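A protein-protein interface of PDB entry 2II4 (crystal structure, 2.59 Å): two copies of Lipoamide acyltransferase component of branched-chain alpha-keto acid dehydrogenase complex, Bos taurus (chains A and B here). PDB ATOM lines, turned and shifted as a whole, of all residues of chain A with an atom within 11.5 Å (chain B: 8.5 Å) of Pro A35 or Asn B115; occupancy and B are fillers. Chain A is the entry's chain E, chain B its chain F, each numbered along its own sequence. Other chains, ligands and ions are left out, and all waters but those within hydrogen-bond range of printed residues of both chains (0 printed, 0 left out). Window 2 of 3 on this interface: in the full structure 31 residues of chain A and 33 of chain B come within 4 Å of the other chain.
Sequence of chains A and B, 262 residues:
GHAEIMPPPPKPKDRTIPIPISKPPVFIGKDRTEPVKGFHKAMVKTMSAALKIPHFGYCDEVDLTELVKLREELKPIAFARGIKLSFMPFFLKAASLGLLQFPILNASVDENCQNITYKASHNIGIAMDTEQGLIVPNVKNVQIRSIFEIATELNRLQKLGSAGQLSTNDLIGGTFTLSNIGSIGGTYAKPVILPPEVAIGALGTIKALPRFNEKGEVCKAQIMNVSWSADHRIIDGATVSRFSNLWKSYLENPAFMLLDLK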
ATOM      1  N   ASP A  31      -4.326 -10.025 -32.736  1.00  0.00           N
ATOM      2  CA  ASP A  31      -4.082 -11.114 -31.803  1.00  0.00           C
ATOM      3  C   ASP A  31      -4.806 -12.365 -32.244  1.00  0.00           C
ATOM      4  O   ASP A  31      -5.876 -12.287 -32.844  1.00  0.00           O
ATOM      5  CB  ASP A  31      -4.600 -10.731 -30.436  1.00  0.00           C
ATOM      6  CG  ASP A  31      -3.732  -9.727 -29.748  1.00  0.00           C
ATOM      7  OD1 ASP A  31      -2.748  -9.180 -30.302  1.00  0.00           O
ATOM      8  OD2 ASP A  31      -4.037  -9.493 -28.592  1.00  0.00           O
ATOM      9  N   ARG A  32      -4.233 -13.519 -31.941  1.00  0.00           N
ATOM     10  CA  ARG A  32      -4.809 -14.774 -32.350  1.00  0.00           C
ATOM     11  C   ARG A  32      -4.720 -15.731 -31.161  1.00  0.00           C
ATOM     12  O   ARG A  32      -3.637 -15.935 -30.609  1.00  0.00           O
ATOM     13  CB  ARG A  32      -4.092 -15.278 -33.613  1.00  0.00           C
ATOM     14  CG  ARG A  32      -4.305 -16.718 -33.986  1.00  0.00           C
ATOM     15  CD  ARG A  32      -3.408 -17.205 -35.195  1.00  0.00           C
ATOM     16  NE  ARG A  32      -1.921 -17.094 -35.095  1.00  0.00           N
ATOM     17  CZ  ARG A  32      -1.050 -18.107 -34.876  1.00  0.00           C
ATOM     18  NH1 ARG A  32      -1.473 -19.363 -34.667  1.00  0.00           N
ATOM     19  NH2 ARG A  32       0.276 -17.866 -34.848  1.00  0.00           N
ATOM     20  N   THR A  33      -5.877 -16.254 -30.741  1.00  0.00           N
ATOM     21  CA  THR A  33      -5.999 -17.263 -29.676  1.00  0.00           C
ATOM     22  C   THR A  33      -6.186 -18.704 -30.213  1.00  0.00           C
ATOM     23  O   THR A  33      -6.852 -18.929 -31.219  1.00  0.00           O
ATOM     24  CB  THR A  33      -7.152 -16.913 -28.707  1.00  0.00           C
ATOM     25  OG1 THR A  33      -6.998 -15.566 -28.237  1.00  0.00           O
ATOM     26  CG2 THR A  33      -7.164 -17.854 -27.518  1.00  0.00           C
ATOM     27  N   GLU A  34      -5.615 -19.683 -29.514  1.00  0.00           N
ATOM     28  CA  GLU A  34      -5.483 -21.036 -30.047  1.00  0.00           C
ATOM     29  C   GLU A  34      -5.318 -22.022 -28.904  1.00  0.00           C
ATOM     30  O   GLU A  34      -4.480 -21.797 -28.035  1.00  0.00           O
ATOM     31  CB  GLU A  34      -4.246 -21.059 -30.926  1.00  0.00           C
ATOM     32  CG  GLU A  34      -4.000 -22.323 -31.636  1.00  0.00           C
ATOM     33  CD  GLU A  34      -3.107 -22.109 -32.845  1.00  0.00           C
ATOM     34  OE1 GLU A  34      -1.929 -22.580 -32.819  1.00  0.00           O
ATOM     35  OE2 GLU A  34      -3.599 -21.450 -33.808  1.00  0.00           O
ATOM     36  N   PRO A  35      -6.082 -23.139 -28.906  1.00  0.00           N
ATOM     37  CA  PRO A  35      -5.988 -24.112 -27.779  1.00  0.00           C
ATOM     38  C   PRO A  35      -4.696 -24.904 -27.767  1.00  0.00           C
ATOM     39  O   PRO A  35      -4.154 -25.224 -28.820  1.00  0.00           O
ATOM     40  CB  PRO A  35      -7.176 -25.063 -27.999  1.00  0.00           C
ATOM     41  CG  PRO A  35      -8.027 -24.397 -29.064  1.00  0.00           C
ATOM     42  CD  PRO A  35      -7.049 -23.598 -29.913  1.00  0.00           C
ATOM     43  N   VAL A  36      -4.194 -25.193 -26.580  1.00  0.00           N
ATOM     44  CA  VAL A  36      -3.065 -26.070 -26.470  1.00  0.00           C
ATOM     45  C   VAL A  36      -3.678 -27.433 -26.717  1.00  0.00           C
ATOM     46  O   VAL A  36      -4.479 -27.930 -25.900  1.00  0.00           O
ATOM     47  CB  VAL A  36      -2.430 -25.991 -25.084  1.00  0.00           C
ATOM     48  CG1 VAL A  36      -1.357 -27.030 -24.934  1.00  0.00           C
ATOM     49  CG2 VAL A  36      -1.857 -24.655 -24.888  1.00  0.00           C
ATOM     50  N   LYS A  37      -3.331 -28.025 -27.854  1.00  0.00           N
ATOM     51  CA  LYS A  37      -3.923 -29.309 -28.207  1.00  0.00           C
ATOM     52  C   LYS A  37      -2.979 -30.518 -28.237  1.00  0.00           C
ATOM     53  O   LYS A  37      -1.763 -30.377 -28.332  1.00  0.00           O
ATOM     54  CB  LYS A  37      -4.738 -29.196 -29.517  1.00  0.00           C
ATOM     55  CG  LYS A  37      -6.209 -28.757 -29.310  1.00  0.00           C
ATOM     56  CD  LYS A  37      -7.061 -29.021 -30.572  1.00  0.00           C
ATOM     57  CE  LYS A  37      -7.064 -27.805 -31.565  1.00  0.00           C
ATOM     58  NZ  LYS A  37      -8.435 -27.186 -31.674  1.00  0.00           N
ATOM     59  N   GLY A  38      -3.586 -31.701 -28.114  1.00  0.00           N
ATOM     60  CA  GLY A  38      -2.948 -33.009 -28.322  1.00  0.00           C
ATOM     61  C   GLY A  38      -1.693 -33.306 -27.530  1.00  0.00           C
ATOM     62  O   GLY A  38      -1.749 -33.512 -26.313  1.00  0.00           O
ATOM     63  N   PHE A  39      -0.570 -33.345 -28.249  1.00  0.00           N
ATOM     64  CA  PHE A  39       0.754 -33.618 -27.672  1.00  0.00           C
ATOM     65  C   PHE A  39       1.268 -32.488 -26.783  1.00  0.00           C
ATOM     66  O   PHE A  39       1.933 -32.730 -25.784  1.00  0.00           O
ATOM     67  CB  PHE A  39       1.805 -33.898 -28.775  1.00  0.00           C
ATOM     68  CG  PHE A  39       3.165 -34.351 -28.228  1.00  0.00           C
ATOM     69  CD1 PHE A  39       3.291 -35.588 -27.526  1.00  0.00           C
ATOM     70  CD2 PHE A  39       4.310 -33.545 -28.402  1.00  0.00           C
ATOM     71  CE1 PHE A  39       4.546 -36.011 -26.996  1.00  0.00           C
ATOM     72  CE2 PHE A  39       5.560 -33.949 -27.879  1.00  0.00           C
ATOM     73  CZ  PHE A  39       5.681 -35.188 -27.166  1.00  0.00           C
ATOM     74  N   HIS A  40       0.969 -31.253 -27.151  1.00  0.00           N
ATOM     75  CA  HIS A  40       1.520 -30.106 -26.447  1.00  0.00           C
ATOM     76  C   HIS A  40       1.051 -30.022 -25.015  1.00  0.00           C
ATOM     77  O   HIS A  40       1.604 -29.254 -24.237  1.00  0.00           O
ATOM     78  CB  HIS A  40       1.220 -28.829 -27.211  1.00  0.00           C
ATOM     79  CG  HIS A  40       1.849 -28.803 -28.564  1.00  0.00           C
ATOM     80  ND1 HIS A  40       3.210 -28.633 -28.745  1.00  0.00           N
ATOM     81  CD2 HIS A  40       1.311 -28.958 -29.799  1.00  0.00           C
ATOM     82  CE1 HIS A  40       3.475 -28.655 -30.039  1.00  0.00           C
ATOM     83  NE2 HIS A  40       2.341 -28.852 -30.700  1.00  0.00           N
ATOM     84  N   LYS A  41       0.048 -30.847 -24.694  1.00  0.00           N
ATOM     85  CA  LYS A  41      -0.576 -30.945 -23.376  1.00  0.00           C
ATOM     86  C   LYS A  41       0.310 -31.744 -22.435  1.00  0.00           C
ATOM     87  O   LYS A  41       0.255 -31.558 -21.231  1.00  0.00           O
ATOM     88  CB  LYS A  41      -1.942 -31.627 -23.487  1.00  0.00           C
ATOM     89  CG  LYS A  41      -3.174 -30.698 -23.599  1.00  0.00           C
ATOM     90  CD  LYS A  41      -4.491 -31.497 -23.821  1.00  0.00           C
ATOM     91  CE  LYS A  41      -5.715 -30.604 -23.572  1.00  0.00           C
ATOM     92  NZ  LYS A  41      -7.037 -31.096 -24.166  1.00  0.00           N
ATOM     93  N   ALA A  42       1.138 -32.625 -22.973  1.00  0.00           N
ATOM     94  CA  ALA A  42       2.006 -33.396 -22.125  1.00  0.00           C
ATOM     95  C   ALA A  42       2.997 -32.474 -21.378  1.00  0.00           C
ATOM     96  O   ALA A  42       3.146 -32.556 -20.143  1.00  0.00           O
ATOM     97  CB  ALA A  42       2.728 -34.440 -22.921  1.00  0.00           C
ATOM     98  N   VAL A  44       2.676 -29.327 -20.719  1.00  0.00           N
ATOM     99  CA  VAL A  44       2.017 -28.449 -19.763  1.00  0.00           C
ATOM    100  C   VAL A  44       1.916 -29.227 -18.431  1.00  0.00           C
ATOM    101  O   VAL A  44       2.233 -28.714 -17.340  1.00  0.00           O
ATOM    102  CB  VAL A  44       0.585 -27.955 -20.233  1.00  0.00           C
ATOM    103  CG1 VAL A  44      -0.060 -27.051 -19.169  1.00  0.00           C
ATOM    104  CG2 VAL A  44       0.625 -27.182 -21.571  1.00  0.00           C
ATOM    105  N   ALA B 107       3.454 -13.866 -26.451  1.00  0.00           N
ATOM    106  CA  ALA B 107       2.163 -14.531 -26.354  1.00  0.00           C
ATOM    107  C   ALA B 107       1.836 -14.641 -24.893  1.00  0.00           C
ATOM    108  O   ALA B 107       2.716 -14.467 -24.065  1.00  0.00           O
ATOM    109  CB  ALA B 107       2.256 -15.911 -26.960  1.00  0.00           C
ATOM    110  N   SER B 108       0.601 -14.978 -24.565  1.00  0.00           N
ATOM    111  CA  SER B 108       0.255 -15.253 -23.174  1.00  0.00           C
ATOM    112  C   SER B 108      -0.510 -16.520 -23.056  1.00  0.00           C
ATOM    113  O   SER B 108      -1.057 -17.092 -24.028  1.00  0.00           O
ATOM    114  CB  SER B 108      -0.563 -14.133 -22.568  1.00  0.00           C
ATOM    115  OG  SER B 108       0.225 -12.960 -22.451  1.00  0.00           O
ATOM    116  N   VAL B 109      -0.564 -16.971 -21.835  1.00  0.00           N
ATOM    117  CA  VAL B 109      -1.243 -18.195 -21.556  1.00  0.00           C
ATOM    118  C   VAL B 109      -2.319 -17.892 -20.511  1.00  0.00           C
ATOM    119  O   VAL B 109      -2.208 -16.915 -19.752  1.00  0.00           O
ATOM    120  CB  VAL B 109      -0.166 -19.194 -21.147  1.00  0.00           C
ATOM    121  CG1 VAL B 109      -0.492 -19.881 -19.878  1.00  0.00           C
ATOM    122  CG2 VAL B 109       0.098 -20.153 -22.274  1.00  0.00           C
ATOM    123  N   ASP B 110      -3.364 -18.701 -20.471  1.00  0.00           N
ATOM    124  CA  ASP B 110      -4.469 -18.469 -19.507  1.00  0.00           C
ATOM    125  C   ASP B 110      -4.336 -19.268 -18.231  1.00  0.00           C
ATOM    126  O   ASP B 110      -3.382 -20.027 -18.077  1.00  0.00           O
ATOM    127  CB  ASP B 110      -5.824 -18.733 -20.158  1.00  0.00           C
ATOM    128  CG  ASP B 110      -5.992 -20.186 -20.638  1.00  0.00           C
ATOM    129  OD1 ASP B 110      -5.041 -20.996 -20.487  1.00  0.00           O
ATOM    130  OD2 ASP B 110      -7.096 -20.517 -21.163  1.00  0.00           O
ATOM    131  N   GLU B 111      -5.301 -19.121 -17.325  1.00  0.00           N
ATOM    132  CA  GLU B 111      -5.086 -19.569 -15.955  1.00  0.00           C
ATOM    133  C   GLU B 111      -4.648 -21.026 -15.915  1.00  0.00           C
ATOM    134  O   GLU B 111      -3.626 -21.322 -15.298  1.00  0.00           O
ATOM    135  CB  GLU B 111      -6.252 -19.228 -14.988  1.00  0.00           C
ATOM    136  CG  GLU B 111      -6.072 -19.754 -13.461  1.00  0.00           C
ATOM    137  CD  GLU B 111      -4.709 -19.347 -12.712  1.00  0.00           C
ATOM    138  OE1 GLU B 111      -3.910 -18.495 -13.221  1.00  0.00           O
ATOM    139  OE2 GLU B 111      -4.436 -19.885 -11.584  1.00  0.00           O
ATOM    140  N   ASN B 112      -5.343 -21.931 -16.605  1.00  0.00           N
ATOM    141  CA  ASN B 112      -4.881 -23.330 -16.571  1.00  0.00           C
ATOM    142  C   ASN B 112      -4.087 -23.811 -17.789  1.00  0.00           C
ATOM    143  O   ASN B 112      -3.893 -25.024 -17.992  1.00  0.00           O
ATOM    144  CB  ASN B 112      -6.022 -24.278 -16.233  1.00  0.00           C
ATOM    145  CG  ASN B 112      -6.620 -23.978 -14.876  1.00  0.00           C
ATOM    146  OD1 ASN B 112      -7.831 -23.817 -14.759  1.00  0.00           O
ATOM    147  ND2 ASN B 112      -5.761 -23.824 -13.847  1.00  0.00           N
ATOM    148  N   CYS B 113      -3.626 -22.842 -18.584  1.00  0.00           N
ATOM    149  CA  CYS B 113      -2.689 -23.090 -19.661  1.00  0.00           C
ATOM    150  C   CYS B 113      -3.267 -24.038 -20.707  1.00  0.00           C
ATOM    151  O   CYS B 113      -2.667 -25.052 -21.078  1.00  0.00           O
ATOM    152  CB  CYS B 113      -1.333 -23.563 -19.119  1.00  0.00           C
ATOM    153  SG  CYS B 113      -0.115 -23.389 -20.369  1.00  0.00           S
ATOM    154  N   GLN B 114      -4.453 -23.674 -21.181  1.00  0.00           N
ATOM    155  CA  GLN B 114      -5.175 -24.483 -22.144  1.00  0.00           C
ATOM    156  C   GLN B 114      -5.319 -23.742 -23.466  1.00  0.00           C
ATOM    157  O   GLN B 114      -5.553 -24.347 -24.504  1.00  0.00           O
ATOM    158  CB  GLN B 114      -6.531 -24.864 -21.585  1.00  0.00           C
ATOM    159  CG  GLN B 114      -6.480 -25.721 -20.318  1.00  0.00           C
ATOM    160  CD  GLN B 114      -7.879 -25.937 -19.706  1.00  0.00           C
ATOM    161  OE1 GLN B 114      -8.162 -26.993 -19.117  1.00  0.00           O
ATOM    162  NE2 GLN B 114      -8.760 -24.943 -19.860  1.00  0.00           N
ATOM    163  N   ASN B 115      -5.147 -22.433 -23.432  1.00  0.00           N
ATOM    164  CA  ASN B 115      -5.191 -21.653 -24.648  1.00  0.00           C
ATOM    165  C   ASN B 115      -4.068 -20.668 -24.640  1.00  0.00           C
ATOM    166  O   ASN B 115      -3.754 -20.125 -23.576  1.00  0.00           O
ATOM    167  CB  ASN B 115      -6.536 -20.907 -24.763  1.00  0.00           C
ATOM    168  CG  ASN B 115      -7.729 -21.814 -24.508  1.00  0.00           C
ATOM    169  OD1 ASN B 115      -8.355 -21.701 -23.468  1.00  0.00           O
ATOM    170  ND2 ASN B 115      -8.006 -22.749 -25.421  1.00  0.00           N
ATOM    171  N   ILE B 116      -3.470 -20.445 -25.808  1.00  0.00           N
ATOM    172  CA  ILE B 116      -2.407 -19.452 -25.977  1.00  0.00           C
ATOM    173  C   ILE B 116      -2.944 -18.292 -26.788  1.00  0.00           C
ATOM    174  O   ILE B 116      -3.605 -18.493 -27.795  1.00  0.00           O
ATOM    175  CB  ILE B 116      -1.174 -20.029 -26.757  1.00  0.00           C
ATOM    176  CG1 ILE B 116      -0.683 -21.315 -26.124  1.00  0.00           C
ATOM    177  CG2 ILE B 116      -0.024 -19.058 -26.770  1.00  0.00           C
ATOM    178  CD1 ILE B 116       0.565 -21.851 -26.765  1.00  0.00           C
ATOM    179  N   THR B 117      -2.641 -17.080 -26.370  1.00  0.00           N
ATOM    180  CA  THR B 117      -2.904 -15.939 -27.188  1.00  0.00           C
ATOM    181  C   THR B 117      -1.560 -15.382 -27.691  1.00  0.00           C
ATOM    182  O   THR B 117      -0.732 -14.913 -26.891  1.00  0.00           O
ATOM    183  CB  THR B 117      -3.689 -14.889 -26.404  1.00  0.00           C
ATOM    184  OG1 THR B 117      -4.928 -15.463 -26.003  1.00  0.00           O
ATOM    185  CG2 THR B 117      -3.954 -13.645 -27.250  1.00  0.00           C
ATOM    186  N   TYR B 118      -1.360 -15.478 -29.021  1.00  0.00           N
ATOM    187  CA  TYR B 118      -0.217 -14.871 -29.755  1.00  0.00           C
ATOM    188  C   TYR B 118      -0.563 -13.405 -29.926  1.00  0.00           C
ATOM    189  O   TYR B 118      -1.645 -13.079 -30.409  1.00  0.00           O
ATOM    190  CB  TYR B 118       0.035 -15.560 -31.120  1.00  0.00           C
ATOM    191  CG  TYR B 118       0.328 -17.074 -31.036  1.00  0.00           C
ATOM    192  CD1 TYR B 118      -0.702 -18.018 -30.830  1.00  0.00           C
ATOM    193  CD2 TYR B 118       1.639 -17.551 -31.137  1.00  0.00           C
ATOM    194  CE1 TYR B 118      -0.417 -19.354 -30.705  1.00  0.00           C
ATOM    195  CE2 TYR B 118       1.923 -18.879 -31.042  1.00  0.00           C
ATOM    196  CZ  TYR B 118       0.904 -19.780 -30.827  1.00  0.00           C
ATOM    197  OH  TYR B 118       1.236 -21.107 -30.741  1.00  0.00           O
ATOM    198  N   VAL B 198       5.384 -14.561 -21.293  1.00  0.00           N
ATOM    199  CA  VAL B 198       5.996 -15.885 -21.269  1.00  0.00           C
ATOM    200  C   VAL B 198       7.528 -15.959 -21.434  1.00  0.00           C
ATOM    201  O   VAL B 198       8.095 -17.070 -21.409  1.00  0.00           O
ATOM    202  CB  VAL B 198       5.364 -16.799 -22.292  1.00  0.00           C
ATOM    203  CG1 VAL B 198       3.879 -17.094 -21.913  1.00  0.00           C
ATOM    204  CG2 VAL B 198       5.560 -16.237 -23.712  1.00  0.00           C
ATOM    205  N   ILE B 234       4.589 -24.013 -22.363  1.00  0.00           N
ATOM    206  CA  ILE B 234       4.387 -23.911 -23.778  1.00  0.00           C
ATOM    207  C   ILE B 234       5.602 -23.627 -24.650  1.00  0.00           C
ATOM    208  O   ILE B 234       5.474 -23.725 -25.881  1.00  0.00           O
ATOM    209  CB  ILE B 234       3.205 -22.994 -24.195  1.00  0.00           C
ATOM    210  CG1 ILE B 234       3.542 -21.502 -24.173  1.00  0.00           C
ATOM    211  CG2 ILE B 234       1.981 -23.374 -23.439  1.00  0.00           C
ATOM    212  CD1 ILE B 234       4.013 -21.006 -22.913  1.00  0.00           C
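The backbone NH of Ile B116 is in hydrogen-bond range of the backbone carbonyl oxygen of Glu A34, at 2.8 Å.
The side-chain hydroxyl (OG1) of Thr B117 is in hydrogen-bond range of the side-chain hydroxyl (OG1) of Thr A33, 3.0 Å away.
O of Arg A32 sits at hydrogen-bond distance from N of Tyr B118 (2.8 Å).
N of Val A36 sits at hydrogen-bond distance from O of Gln B114.
Among the printed residues, merely in contact across the chains: Asp A31 with Tyr B118, Arg A32 with Ile B116, Arg A32 with Thr B117, Thr A33 with Ile B116, Glu A34 with Asn B115, Pro A35 with Gln B114, Pro A35 with Asn B115, Val A36 with Cys B113, Val A36 with Ile B116 and Val A44 with Cys B113.
Along chain A the printed residues that touch a printed residue of chain B span positions 31 to 44.
OD1 of Asp B110 sits at hydrogen-bond distance from N of Cys B113 (3.0 Å).
The side-chain carboxylate of Asp B110 sits at hydrogen-bond distance from the backbone NH of Gln B114 (2.8 Å).
NH1 of Arg A32 is in salt-bridge range of OE2 of Glu A34 (3.1 Å).
The backbone NH of Ser B108 lies within hydrogen-bond range of the backbone carbonyl oxygen of Thr B117 (2.7 Å).
The side-chain amide oxygen of Asn B115 lies close to the side-chain carboxylate of Asp B110, 2.9 Å away.
Printed residues of chain B within 4 Å of Asp A31: Tyr B118 (3.4 Å).
Printed residues of chain B within 4 Å of Arg A32: Ile B116, Thr B117 and Tyr B118.
Printed residues of chain B within 4 Å of Glu A34: Asn B115 and Ile B116.
Of the printed residues of chain B, Pro A35 touches Gln B114 (3.3 Å) and Asn B115 (3.4 Å).
Printed residues of chain B within 4 Å of Val A36: Cys B113 (3.9 Å), Gln B114 (2.6 Å) and Ile B116 (3.7 Å).
Of the printed residues of chain B, Val A44 touches Cys B113.
No residue of chain A comes within 4 Å of Val B109.
Gln B114 touches two residues of chain A.
Of chain A, only Glu A34 (3.5 Å) and Pro A35 (3.4 Å) come within 4 Å of Asn B115.
The nearest residue of chain B that does not touch Pro A35 is Ile B116 (4.9 Å).
No position is printed for both chains.
Of the 14 pairs that touch across the chains among the printed residues, none has its exchanged pair printed and touching as well.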
